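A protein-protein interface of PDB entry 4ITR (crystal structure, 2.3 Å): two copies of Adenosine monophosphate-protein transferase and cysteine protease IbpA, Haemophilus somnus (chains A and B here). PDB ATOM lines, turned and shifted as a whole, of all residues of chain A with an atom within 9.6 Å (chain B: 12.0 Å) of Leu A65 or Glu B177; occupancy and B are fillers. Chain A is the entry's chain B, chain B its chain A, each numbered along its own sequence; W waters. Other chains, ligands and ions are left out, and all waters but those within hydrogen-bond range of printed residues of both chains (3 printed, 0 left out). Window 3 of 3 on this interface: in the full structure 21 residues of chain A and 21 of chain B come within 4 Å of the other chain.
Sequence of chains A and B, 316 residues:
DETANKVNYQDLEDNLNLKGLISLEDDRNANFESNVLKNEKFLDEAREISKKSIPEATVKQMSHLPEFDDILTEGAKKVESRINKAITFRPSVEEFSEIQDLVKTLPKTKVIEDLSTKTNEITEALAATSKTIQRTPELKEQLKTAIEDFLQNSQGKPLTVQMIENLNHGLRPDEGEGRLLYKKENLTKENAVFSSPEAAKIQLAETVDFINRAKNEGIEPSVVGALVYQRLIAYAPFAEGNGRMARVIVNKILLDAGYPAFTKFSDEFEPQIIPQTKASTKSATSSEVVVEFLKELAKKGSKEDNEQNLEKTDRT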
ATOM      1  N   ARG A  47     -12.756  37.273 -11.877  1.00  0.00           N
ATOM      2  CA  ARG A  47     -12.322  36.545 -10.689  1.00  0.00           C
ATOM      3  C   ARG A  47     -11.696  37.481  -9.659  1.00  0.00           C
ATOM      4  O   ARG A  47     -11.936  37.342  -8.460  1.00  0.00           O
ATOM      5  CB  ARG A  47     -11.323  35.445 -11.068  1.00  0.00           C
ATOM      6  CG  ARG A  47     -11.892  34.327 -11.924  1.00  0.00           C
ATOM      7  CD  ARG A  47     -10.795  33.395 -12.424  1.00  0.00           C
ATOM      8  NE  ARG A  47     -11.314  32.362 -13.321  1.00  0.00           N
ATOM      9  CZ  ARG A  47     -10.833  32.109 -14.535  1.00  0.00           C
ATOM     10  NH1 ARG A  47      -9.815  32.812 -15.012  1.00  0.00           N
ATOM     11  NH2 ARG A  47     -11.372  31.152 -15.275  1.00  0.00           N
ATOM     12  N   LYS A  51     -13.353  38.530  -5.899  1.00  0.00           N
ATOM     13  CA  LYS A  51     -12.613  38.149  -4.696  1.00  0.00           C
ATOM     14  C   LYS A  51     -12.353  39.310  -3.740  1.00  0.00           C
ATOM     15  O   LYS A  51     -12.101  39.094  -2.552  1.00  0.00           O
ATOM     16  CB  LYS A  51     -11.278  37.493  -5.068  1.00  0.00           C
ATOM     17  CG  LYS A  51     -11.367  36.000  -5.384  1.00  0.00           C
ATOM     18  CD  LYS A  51      -9.996  35.421  -5.729  1.00  0.00           C
ATOM     19  CE  LYS A  51     -10.070  33.914  -5.948  1.00  0.00           C
ATOM     20  NZ  LYS A  51      -8.776  33.322  -6.410  1.00  0.00           N
ATOM     21  N   THR A  58     -12.946  32.699   3.654  1.00  0.00           N
ATOM     22  CA  THR A  58     -14.055  32.193   2.850  1.00  0.00           C
ATOM     23  C   THR A  58     -13.559  31.770   1.463  1.00  0.00           C
ATOM     24  O   THR A  58     -13.995  30.748   0.923  1.00  0.00           O
ATOM     25  CB  THR A  58     -15.184  33.238   2.723  1.00  0.00           C
ATOM     26  OG1 THR A  58     -15.747  33.494   4.017  1.00  0.00           O
ATOM     27  CG2 THR A  58     -16.280  32.740   1.791  1.00  0.00           C
ATOM     28  N   VAL A  59     -12.646  32.555   0.896  1.00  0.00           N
ATOM     29  CA  VAL A  59     -12.008  32.199  -0.369  1.00  0.00           C
ATOM     30  C   VAL A  59     -11.283  30.863  -0.234  1.00  0.00           C
ATOM     31  O   VAL A  59     -11.367  30.010  -1.121  1.00  0.00           O
ATOM     32  CB  VAL A  59     -11.001  33.276  -0.823  1.00  0.00           C
ATOM     33  CG1 VAL A  59     -10.283  32.838  -2.094  1.00  0.00           C
ATOM     34  CG2 VAL A  59     -11.699  34.605  -1.044  1.00  0.00           C
ATOM     35  N   LYS A  60     -10.580  30.688   0.883  1.00  0.00           N
ATOM     36  CA  LYS A  60      -9.865  29.443   1.157  1.00  0.00           C
ATOM     37  C   LYS A  60     -10.825  28.257   1.187  1.00  0.00           C
ATOM     38  O   LYS A  60     -10.531  27.199   0.632  1.00  0.00           O
ATOM     39  CB  LYS A  60      -9.113  29.523   2.489  1.00  0.00           C
ATOM     40  CG  LYS A  60      -8.049  30.610   2.572  1.00  0.00           C
ATOM     41  CD  LYS A  60      -6.936  30.410   1.558  1.00  0.00           C
ATOM     42  CE  LYS A  60      -5.944  31.572   1.587  1.00  0.00           C
ATOM     43  NZ  LYS A  60      -5.304  31.759   2.921  1.00  0.00           N
ATOM     44  N   GLN A  61     -11.972  28.440   1.835  1.00  0.00           N
ATOM     45  CA  GLN A  61     -12.987  27.395   1.918  1.00  0.00           C
ATOM     46  C   GLN A  61     -13.565  27.077   0.540  1.00  0.00           C
ATOM     47  O   GLN A  61     -13.656  25.913   0.147  1.00  0.00           O
ATOM     48  CB  GLN A  61     -14.105  27.812   2.882  1.00  0.00           C
ATOM     49  CG  GLN A  61     -13.672  27.910   4.348  1.00  0.00           C
ATOM     50  CD  GLN A  61     -14.751  28.494   5.250  1.00  0.00           C
ATOM     51  OE1 GLN A  61     -15.561  29.317   4.821  1.00  0.00           O
ATOM     52  NE2 GLN A  61     -14.762  28.069   6.507  1.00  0.00           N
ATOM     53  N   MET A  62     -13.938  28.123  -0.193  1.00  0.00           N
ATOM     54  CA  MET A  62     -14.563  27.976  -1.505  1.00  0.00           C
ATOM     55  C   MET A  62     -13.672  27.309  -2.552  1.00  0.00           C
ATOM     56  O   MET A  62     -14.172  26.646  -3.462  1.00  0.00           O
ATOM     57  CB  MET A  62     -15.036  29.340  -2.010  1.00  0.00           C
ATOM     58  CG  MET A  62     -16.242  29.872  -1.263  1.00  0.00           C
ATOM     59  SD  MET A  62     -17.680  28.820  -1.514  1.00  0.00           S
ATOM     60  CE  MET A  62     -18.310  28.758   0.156  1.00  0.00           C
ATOM     61  N   SER A  63     -12.358  27.468  -2.415  1.00  0.00           N
ATOM     62  CA  SER A  63     -11.417  26.916  -3.391  1.00  0.00           C
ATOM     63  C   SER A  63     -11.462  25.389  -3.437  1.00  0.00           C
ATOM     64  O   SER A  63     -10.931  24.771  -4.362  1.00  0.00           O
ATOM     65  CB  SER A  63      -9.992  27.387  -3.096  1.00  0.00           C
ATOM     66  OG  SER A  63      -9.503  26.811  -1.898  1.00  0.00           O
ATOM     67  N   HIS A  64     -12.098  24.791  -2.433  1.00  0.00           N
ATOM     68  CA  HIS A  64     -12.263  23.344  -2.367  1.00  0.00           C
ATOM     69  C   HIS A  64     -13.532  22.895  -3.089  1.00  0.00           C
ATOM     70  O   HIS A  64     -13.726  21.704  -3.339  1.00  0.00           O
ATOM     71  CB  HIS A  64     -12.315  22.885  -0.907  1.00  0.00           C
ATOM     72  CG  HIS A  64     -11.052  23.143  -0.142  1.00  0.00           C
ATOM     73  ND1 HIS A  64      -9.957  22.310  -0.214  1.00  0.00           N
ATOM     74  CD2 HIS A  64     -10.719  24.131   0.721  1.00  0.00           C
ATOM     75  CE1 HIS A  64      -8.999  22.780   0.566  1.00  0.00           C
ATOM     76  NE2 HIS A  64      -9.435  23.884   1.142  1.00  0.00           N
ATOM     77  N   LEU A  65     -14.394  23.856  -3.418  1.00  0.00           N
ATOM     78  CA  LEU A  65     -15.679  23.554  -4.046  1.00  0.00           C
ATOM     79  C   LEU A  65     -15.648  23.758  -5.562  1.00  0.00           C
ATOM     80  O   LEU A  65     -15.144  24.770  -6.048  1.00  0.00           O
ATOM     81  CB  LEU A  65     -16.793  24.391  -3.414  1.00  0.00           C
ATOM     82  CG  LEU A  65     -16.935  24.237  -1.897  1.00  0.00           C
ATOM     83  CD1 LEU A  65     -18.135  24.999  -1.364  1.00  0.00           C
ATOM     84  CD2 LEU A  65     -17.030  22.773  -1.516  1.00  0.00           C
ATOM     85  N   PRO A  66     -16.200  22.792  -6.313  1.00  0.00           N
ATOM     86  CA  PRO A  66     -16.160  22.763  -7.783  1.00  0.00           C
ATOM     87  C   PRO A  66     -16.884  23.938  -8.445  1.00  0.00           C
ATOM     88  O   PRO A  66     -16.604  24.252  -9.602  1.00  0.00           O
ATOM     89  CB  PRO A  66     -16.891  21.460  -8.128  1.00  0.00           C
ATOM     90  CG  PRO A  66     -16.824  20.631  -6.887  1.00  0.00           C
ATOM     91  CD  PRO A  66     -16.883  21.609  -5.759  1.00  0.00           C
ATOM     92  N   GLU A  67     -17.801  24.574  -7.723  1.00  0.00           N
ATOM     93  CA  GLU A  67     -18.641  25.616  -8.307  1.00  0.00           C
ATOM     94  C   GLU A  67     -18.082  27.032  -8.140  1.00  0.00           C
ATOM     95  O   GLU A  67     -18.660  27.991  -8.654  1.00  0.00           O
ATOM     96  CB  GLU A  67     -20.056  25.538  -7.725  1.00  0.00           C
ATOM     97  CG  GLU A  67     -20.837  24.301  -8.152  1.00  0.00           C
ATOM     98  CD  GLU A  67     -22.169  24.163  -7.432  1.00  0.00           C
ATOM     99  OE1 GLU A  67     -22.682  25.180  -6.918  1.00  0.00           O
ATOM    100  OE2 GLU A  67     -22.698  23.032  -7.379  1.00  0.00           O
ATOM    101  N   PHE A  68     -16.954  27.156  -7.444  1.00  0.00           N
ATOM    102  CA  PHE A  68     -16.399  28.464  -7.086  1.00  0.00           C
ATOM    103  C   PHE A  68     -16.114  29.370  -8.285  1.00  0.00           C
ATOM    104  O   PHE A  68     -16.496  30.540  -8.278  1.00  0.00           O
ATOM    105  CB  PHE A  68     -15.129  28.308  -6.244  1.00  0.00           C
ATOM    106  CG  PHE A  68     -14.689  29.578  -5.567  1.00  0.00           C
ATOM    107  CD1 PHE A  68     -15.616  30.549  -5.213  1.00  0.00           C
ATOM    108  CD2 PHE A  68     -13.348  29.806  -5.298  1.00  0.00           C
ATOM    109  CE1 PHE A  68     -15.214  31.718  -4.589  1.00  0.00           C
ATOM    110  CE2 PHE A  68     -12.938  30.975  -4.678  1.00  0.00           C
ATOM    111  CZ  PHE A  68     -13.872  31.932  -4.325  1.00  0.00           C
ATOM    112  N   ASP A  69     -15.446  28.838  -9.306  1.00  0.00           N
ATOM    113  CA  ASP A  69     -15.069  29.658 -10.458  1.00  0.00           C
ATOM    114  C   ASP A  69     -16.295  30.212 -11.183  1.00  0.00           C
ATOM    115  O   ASP A  69     -16.311  31.378 -11.588  1.00  0.00           O
ATOM    116  CB  ASP A  69     -14.187  28.872 -11.435  1.00  0.00           C
ATOM    117  CG  ASP A  69     -13.410  29.777 -12.380  1.00  0.00           C
ATOM    118  OD1 ASP A  69     -12.770  30.738 -11.898  1.00  0.00           O
ATOM    119  OD2 ASP A  69     -13.444  29.536 -13.607  1.00  0.00           O
ATOM    120  N   ASP A  70     -17.320  29.379 -11.337  1.00  0.00           N
ATOM    121  CA  ASP A  70     -18.556  29.806 -11.985  1.00  0.00           C
ATOM    122  C   ASP A  70     -19.292  30.863 -11.162  1.00  0.00           C
ATOM    123  O   ASP A  70     -19.832  31.818 -11.718  1.00  0.00           O
ATOM    124  CB  ASP A  70     -19.466  28.606 -12.271  1.00  0.00           C
ATOM    125  CG  ASP A  70     -19.094  27.884 -13.553  1.00  0.00           C
ATOM    126  OD1 ASP A  70     -18.233  28.395 -14.301  1.00  0.00           O
ATOM    127  OD2 ASP A  70     -19.676  26.810 -13.820  1.00  0.00           O
ATOM    128  N   ILE A  71     -19.307  30.691  -9.843  1.00  0.00           N
ATOM    129  CA  ILE A  71     -19.871  31.695  -8.942  1.00  0.00           C
ATOM    130  C   ILE A  71     -19.140  33.027  -9.124  1.00  0.00           C
ATOM    131  O   ILE A  71     -19.749  34.097  -9.100  1.00  0.00           O
ATOM    132  CB  ILE A  71     -19.772  31.244  -7.462  1.00  0.00           C
ATOM    133  CG1 ILE A  71     -20.646  30.011  -7.215  1.00  0.00           C
ATOM    134  CG2 ILE A  71     -20.182  32.367  -6.519  1.00  0.00           C
ATOM    135  CD1 ILE A  71     -20.577  29.477  -5.794  1.00  0.00           C
ATOM    136  N   LEU A  72     -17.830  32.943  -9.330  1.00  0.00           N
ATOM    137  CA  LEU A  72     -16.986  34.120  -9.513  1.00  0.00           C
ATOM    138  C   LEU A  72     -17.276  34.860 -10.819  1.00  0.00           C
ATOM    139  O   LEU A  72     -17.250  36.093 -10.865  1.00  0.00           O
ATOM    140  CB  LEU A  72     -15.514  33.704  -9.469  1.00  0.00           C
ATOM    141  CG  LEU A  72     -14.701  34.049  -8.224  1.00  0.00           C
ATOM    142  CD1 LEU A  72     -15.590  34.127  -7.005  1.00  0.00           C
ATOM    143  CD2 LEU A  72     -13.582  33.039  -8.004  1.00  0.00           C
ATOM    144  N   GLU B 138       0.964  10.899  -7.808  1.00  0.00           N
ATOM    145  CA  GLU B 138      -0.297  11.542  -8.169  1.00  0.00           C
ATOM    146  C   GLU B 138      -0.045  12.824  -8.958  1.00  0.00           C
ATOM    147  O   GLU B 138      -0.720  13.098  -9.952  1.00  0.00           O
ATOM    148  CB  GLU B 138      -1.119  11.854  -6.915  1.00  0.00           C
ATOM    149  CG  GLU B 138      -2.415  12.610  -7.190  1.00  0.00           C
ATOM    150  CD  GLU B 138      -3.194  12.922  -5.926  1.00  0.00           C
ATOM    151  OE1 GLU B 138      -3.919  13.939  -5.912  1.00  0.00           O
ATOM    152  OE2 GLU B 138      -3.086  12.149  -4.950  1.00  0.00           O
ATOM    153  N   GLN B 142      -0.617  13.549 -13.060  1.00  0.00           N
ATOM    154  CA  GLN B 142      -1.444  14.681 -13.471  1.00  0.00           C
ATOM    155  C   GLN B 142      -0.739  15.526 -14.527  1.00  0.00           C
ATOM    156  O   GLN B 142      -1.339  15.909 -15.530  1.00  0.00           O
ATOM    157  CB  GLN B 142      -1.784  15.559 -12.266  1.00  0.00           C
ATOM    158  CG  GLN B 142      -2.851  14.999 -11.339  1.00  0.00           C
ATOM    159  CD  GLN B 142      -2.906  15.740 -10.015  1.00  0.00           C
ATOM    160  OE1 GLN B 142      -1.873  16.066  -9.430  1.00  0.00           O
ATOM    161  NE2 GLN B 142      -4.115  16.015  -9.540  1.00  0.00           N
ATOM    162  N   HIS B 169      -2.706  25.664 -17.176  1.00  0.00           N
ATOM    163  CA  HIS B 169      -3.722  25.244 -16.214  1.00  0.00           C
ATOM    164  C   HIS B 169      -3.539  23.776 -15.849  1.00  0.00           C
ATOM    165  O   HIS B 169      -3.657  23.395 -14.682  1.00  0.00           O
ATOM    166  CB  HIS B 169      -5.132  25.470 -16.765  1.00  0.00           C
ATOM    167  CG  HIS B 169      -6.224  25.074 -15.817  1.00  0.00           C
ATOM    168  ND1 HIS B 169      -6.542  25.812 -14.696  1.00  0.00           N
ATOM    169  CD2 HIS B 169      -7.076  24.021 -15.825  1.00  0.00           C
ATOM    170  CE1 HIS B 169      -7.539  25.231 -14.055  1.00  0.00           C
ATOM    171  NE2 HIS B 169      -7.882  24.141 -14.718  1.00  0.00           N
ATOM    172  N   GLY B 170      -3.252  22.956 -16.854  1.00  0.00           N
ATOM    173  CA  GLY B 170      -3.011  21.541 -16.633  1.00  0.00           C
ATOM    174  C   GLY B 170      -1.781  21.291 -15.780  1.00  0.00           C
ATOM    175  O   GLY B 170      -1.699  20.284 -15.072  1.00  0.00           O
ATOM    176  N   ARG B 172      -0.884  23.069 -13.301  1.00  0.00           N
ATOM    177  CA  ARG B 172      -1.132  23.616 -11.966  1.00  0.00           C
ATOM    178  C   ARG B 172      -2.276  22.886 -11.248  1.00  0.00           C
ATOM    179  O   ARG B 172      -3.284  23.503 -10.904  1.00  0.00           O
ATOM    180  CB  ARG B 172      -1.447  25.113 -12.066  1.00  0.00           C
ATOM    181  CG  ARG B 172      -0.284  25.965 -12.563  1.00  0.00           C
ATOM    182  CD  ARG B 172      -0.746  27.277 -13.189  1.00  0.00           C
ATOM    183  NE  ARG B 172      -1.559  28.087 -12.283  1.00  0.00           N
ATOM    184  CZ  ARG B 172      -1.992  29.313 -12.562  1.00  0.00           C
ATOM    185  NH1 ARG B 172      -1.683  29.879 -13.722  1.00  0.00           N
ATOM    186  NH2 ARG B 172      -2.727  29.979 -11.684  1.00  0.00           N
ATOM    187  N   PRO B 173      -2.111  21.573 -10.994  1.00  0.00           N
ATOM    188  CA  PRO B 173      -3.223  20.750 -10.500  1.00  0.00           C
ATOM    189  C   PRO B 173      -3.498  20.870  -8.994  1.00  0.00           C
ATOM    190  O   PRO B 173      -4.623  20.605  -8.565  1.00  0.00           O
ATOM    191  CB  PRO B 173      -2.767  19.328 -10.841  1.00  0.00           C
ATOM    192  CG  PRO B 173      -1.283  19.389 -10.738  1.00  0.00           C
ATOM    193  CD  PRO B 173      -0.877  20.781 -11.164  1.00  0.00           C
ATOM    194  N   ASP B 174      -2.498  21.264  -8.212  1.00  0.00           N
ATOM    195  CA  ASP B 174      -2.633  21.309  -6.755  1.00  0.00           C
ATOM    196  C   ASP B 174      -3.128  22.662  -6.242  1.00  0.00           C
ATOM    197  O   ASP B 174      -2.884  23.016  -5.089  1.00  0.00           O
ATOM    198  CB  ASP B 174      -1.286  21.003  -6.091  1.00  0.00           C
ATOM    199  CG  ASP B 174      -0.626  19.756  -6.646  1.00  0.00           C
ATOM    200  OD1 ASP B 174       0.623  19.687  -6.623  1.00  0.00           O
ATOM    201  OD2 ASP B 174      -1.352  18.848  -7.103  1.00  0.00           O
ATOM    202  N   GLU B 175      -3.835  23.405  -7.088  1.00  0.00           N
ATOM    203  CA  GLU B 175      -4.088  24.824  -6.828  1.00  0.00           C
ATOM    204  C   GLU B 175      -5.370  25.172  -6.066  1.00  0.00           C
ATOM    205  O   GLU B 175      -5.379  26.094  -5.246  1.00  0.00           O
ATOM    206  CB  GLU B 175      -4.055  25.610  -8.142  1.00  0.00           C
ATOM    207  CG  GLU B 175      -2.830  26.493  -8.309  1.00  0.00           C
ATOM    208  CD  GLU B 175      -2.980  27.470  -9.454  1.00  0.00           C
ATOM    209  OE1 GLU B 175      -2.292  28.511  -9.438  1.00  0.00           O
ATOM    210  OE2 GLU B 175      -3.789  27.200 -10.367  1.00  0.00           O
ATOM    211  N   GLY B 176      -6.451  24.454  -6.348  1.00  0.00           N
ATOM    212  CA  GLY B 176      -7.755  24.824  -5.830  1.00  0.00           C
ATOM    213  C   GLY B 176      -8.554  25.535  -6.905  1.00  0.00           C
ATOM    214  O   GLY B 176      -8.038  25.792  -7.994  1.00  0.00           O
ATOM    215  N   GLU B 177      -9.808  25.860  -6.606  1.00  0.00           N
ATOM    216  CA  GLU B 177     -10.682  26.483  -7.593  1.00  0.00           C
ATOM    217  C   GLU B 177     -10.624  28.008  -7.534  1.00  0.00           C
ATOM    218  O   GLU B 177     -10.275  28.582  -6.503  1.00  0.00           O
ATOM    219  CB  GLU B 177     -12.123  26.008  -7.396  1.00  0.00           C
ATOM    220  CG  GLU B 177     -12.287  24.496  -7.445  1.00  0.00           C
ATOM    221  CD  GLU B 177     -11.969  23.918  -8.809  1.00  0.00           C
ATOM    222  OE1 GLU B 177     -11.384  22.816  -8.865  1.00  0.00           O
ATOM    223  OE2 GLU B 177     -12.310  24.561  -9.825  1.00  0.00           O
ATOM    224  N   GLY B 178     -10.953  28.658  -8.648  1.00  0.00           N
ATOM    225  CA  GLY B 178     -11.080  30.105  -8.685  1.00  0.00           C
ATOM    226  C   GLY B 178      -9.786  30.897  -8.757  1.00  0.00           C
ATOM    227  O   GLY B 178      -9.798  32.123  -8.617  1.00  0.00           O
ATOM    228  N   ARG B 179      -8.671  30.208  -8.977  1.00  0.00           N
ATOM    229  CA  ARG B 179      -7.383  30.882  -9.100  1.00  0.00           C
ATOM    230  C   ARG B 179      -7.300  31.649 -10.419  1.00  0.00           C
ATOM    231  O   ARG B 179      -7.862  31.224 -11.431  1.00  0.00           O
ATOM    232  CB  ARG B 179      -6.231  29.877  -9.008  1.00  0.00           C
ATOM    233  CG  ARG B 179      -6.324  28.908  -7.832  1.00  0.00           C
ATOM    234  CD  ARG B 179      -6.530  29.641  -6.512  1.00  0.00           C
ATOM    235  NE  ARG B 179      -5.519  30.671  -6.284  1.00  0.00           N
ATOM    236  CZ  ARG B 179      -4.343  30.448  -5.706  1.00  0.00           C
ATOM    237  NH1 ARG B 179      -4.023  29.228  -5.300  1.00  0.00           N
ATOM    238  NH2 ARG B 179      -3.483  31.444  -5.537  1.00  0.00           N
ATOM    239  N   LEU B 180      -6.612  32.787 -10.400  1.00  0.00           N
ATOM    240  CA  LEU B 180      -6.353  33.544 -11.622  1.00  0.00           C
ATOM    241  C   LEU B 180      -5.347  32.780 -12.468  1.00  0.00           C
ATOM    242  O   LEU B 180      -4.388  32.220 -11.936  1.00  0.00           O
ATOM    243  CB  LEU B 180      -5.780  34.921 -11.286  1.00  0.00           C
ATOM    244  CG  LEU B 180      -6.486  35.758 -10.221  1.00  0.00           C
ATOM    245  CD1 LEU B 180      -5.720  37.040  -9.957  1.00  0.00           C
ATOM    246  CD2 LEU B 180      -7.891  36.074 -10.656  1.00  0.00           C
ATOM    247  N   LEU B 181      -5.560  32.749 -13.780  1.00  0.00           N
ATOM    248  CA  LEU B 181      -4.611  32.097 -14.678  1.00  0.00           C
ATOM    249  C   LEU B 181      -3.349  32.940 -14.825  1.00  0.00           C
ATOM    250  O   LEU B 181      -2.238  32.476 -14.551  1.00  0.00           O
ATOM    251  CB  LEU B 181      -5.241  31.850 -16.053  1.00  0.00           C
ATOM    252  CG  LEU B 181      -4.303  31.167 -17.052  1.00  0.00           C
ATOM    253  CD1 LEU B 181      -3.879  29.811 -16.530  1.00  0.00           C
ATOM    254  CD2 LEU B 181      -4.935  31.025 -18.418  1.00  0.00           C
ATOM    255  N   ALA B 239       0.353  33.246 -13.240  1.00  0.00           N
ATOM    256  CA  ALA B 239       0.544  33.366 -11.798  1.00  0.00           C
ATOM    257  C   ALA B 239       1.469  32.275 -11.277  1.00  0.00           C
ATOM    258  O   ALA B 239       2.181  32.462 -10.286  1.00  0.00           O
ATOM    259  CB  ALA B 239      -0.793  33.301 -11.091  1.00  0.00           C
ATOM    260  N   GLU B 240       1.449  31.135 -11.959  1.00  0.00           N
ATOM    261  CA  GLU B 240       2.200  29.965 -11.531  1.00  0.00           C
ATOM    262  C   GLU B 240       2.550  29.083 -12.728  1.00  0.00           C
ATOM    263  O   GLU B 240       1.947  29.205 -13.799  1.00  0.00           O
ATOM    264  CB  GLU B 240       1.361  29.161 -10.535  1.00  0.00           C
ATOM    265  CG  GLU B 240       2.137  28.603  -9.358  1.00  0.00           C
ATOM    266  CD  GLU B 240       2.376  29.632  -8.275  1.00  0.00           C
ATOM    267  OE1 GLU B 240       1.430  30.370  -7.921  1.00  0.00           O
ATOM    268  OE2 GLU B 240       3.513  29.696  -7.769  1.00  0.00           O
HETATM  269  O   HOH W   1     -14.685  25.830  -9.717  1.00  0.00           O
HETATM  270  O   HOH W   2      -9.363  30.684  -5.305  1.00  0.00           O
HETATM  271  O   HOH W   3      -9.934  29.202 -12.420  1.00  0.00           O
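The backbone carbonyl oxygen of Ser A63 is in hydrogen-bond range of the backbone NH of Glu B177 (2.7 Å). The backbone carbonyl oxygen (O) of Gly B178 is in hydrogen-bond range of the side-chain amino group (NZ) of Lys A51, at 2.7 Å.
The guanidinium group (NH2) of Arg B172 is in hydrogen-bond range of the backbone carbonyl oxygen (O) of Leu B180, 2.8 Å away. NH1 of Arg B179 lies within hydrogen-bond range of O of Glu B175. OD1 of Asp A69 lies within salt-bridge range of NE of Arg A47 (2.6 Å). O of Lys A60 lies within hydrogen-bond range of OG of Ser A63 (2.8 Å).
Arg B179 touches Arg A47. CB of Arg A47 touches CD2 of Leu B180, 3.5 Å away. CA of Arg B179 touches NZ of Lys A51, 3.9 Å away. Ser A63 touches Gly B176 (O to CA, 3.5 Å). Leu A65 touches Glu B177. Glu B177 touches Phe A68 (O to CD2, 3.5 Å). OD1 of Asp A69 touches CA of Gly B178 (3.7 Å). Gly B178 touches Leu A72 (CA to CD2, 3.9 Å).
Printed residues of chain B within 4 Å of Leu A65: Glu B177 (3.2 Å). No residue of chain B comes within 4 Å of Met A62. Printed residues of chain B within 4 Å of Ser A63: Gly B176 (3.5 Å) and Glu B177 (2.7 Å). No residue of chain B comes within 4 Å of His A64. Phe A68 touches one residue of chain B. Of chain B, only Gly B178 (3.7 Å) comes within 4 Å of Asp A69. Gly B176 touches just one residue of chain A: Ser A63 (3.5 Å). Gly B178 touches just these residues of chain A: Lys A51 (2.7 Å), Asp A69 (3.7 Å) and Leu A72 (3.9 Å). Of the printed residues of chain B, Leu A72 touches Gly B178 (3.9 Å). Of the printed residues of chain A, Arg B179 touches Arg A47 (3.8 Å) and Lys A51 (3.9 Å). Printed residues of chain B within 4 Å of Lys A51: Gly B178 and Arg B179. The nearest residue of chain B that does not touch Leu A65 is Gly B178 (6.3 Å). The nearest residue of chain A that does not touch Glu B177 is Pro A66 (4.3 Å).
Hydrophobic or aromatic side chains of chain A that line the printed part of chain B: Phe A68 and Leu A72. Printed residues of chain B that touch a printed residue of chain A: Gly B176, Glu B177, Gly B178, Arg B179 and Leu B180. Among the printed residues, 10 pairs touch across the chains. Among the printed residues, no Asp or Glu carboxylate lies within 4 Å of a Lys or Arg side-chain nitrogen of the other chain.
No position is printed for both chains.
Water W1 lies within hydrogen-bond range of the backbone carbonyl oxygen of Pro A66 (2.5 Å), the side-chain carboxylate of Glu B177 (2.7 Å), the backbone NH of Asp A69 (3.1 Å) and the backbone NH of Phe A68 (3.5 Å). Water W2 lies within hydrogen-bond range of O of Glu B177 (2.6 Å) and NZ of Lys A51 (2.9 Å). Water W3 lies within hydrogen-bond range of O of Arg B179 and OD1 of Asp A69.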
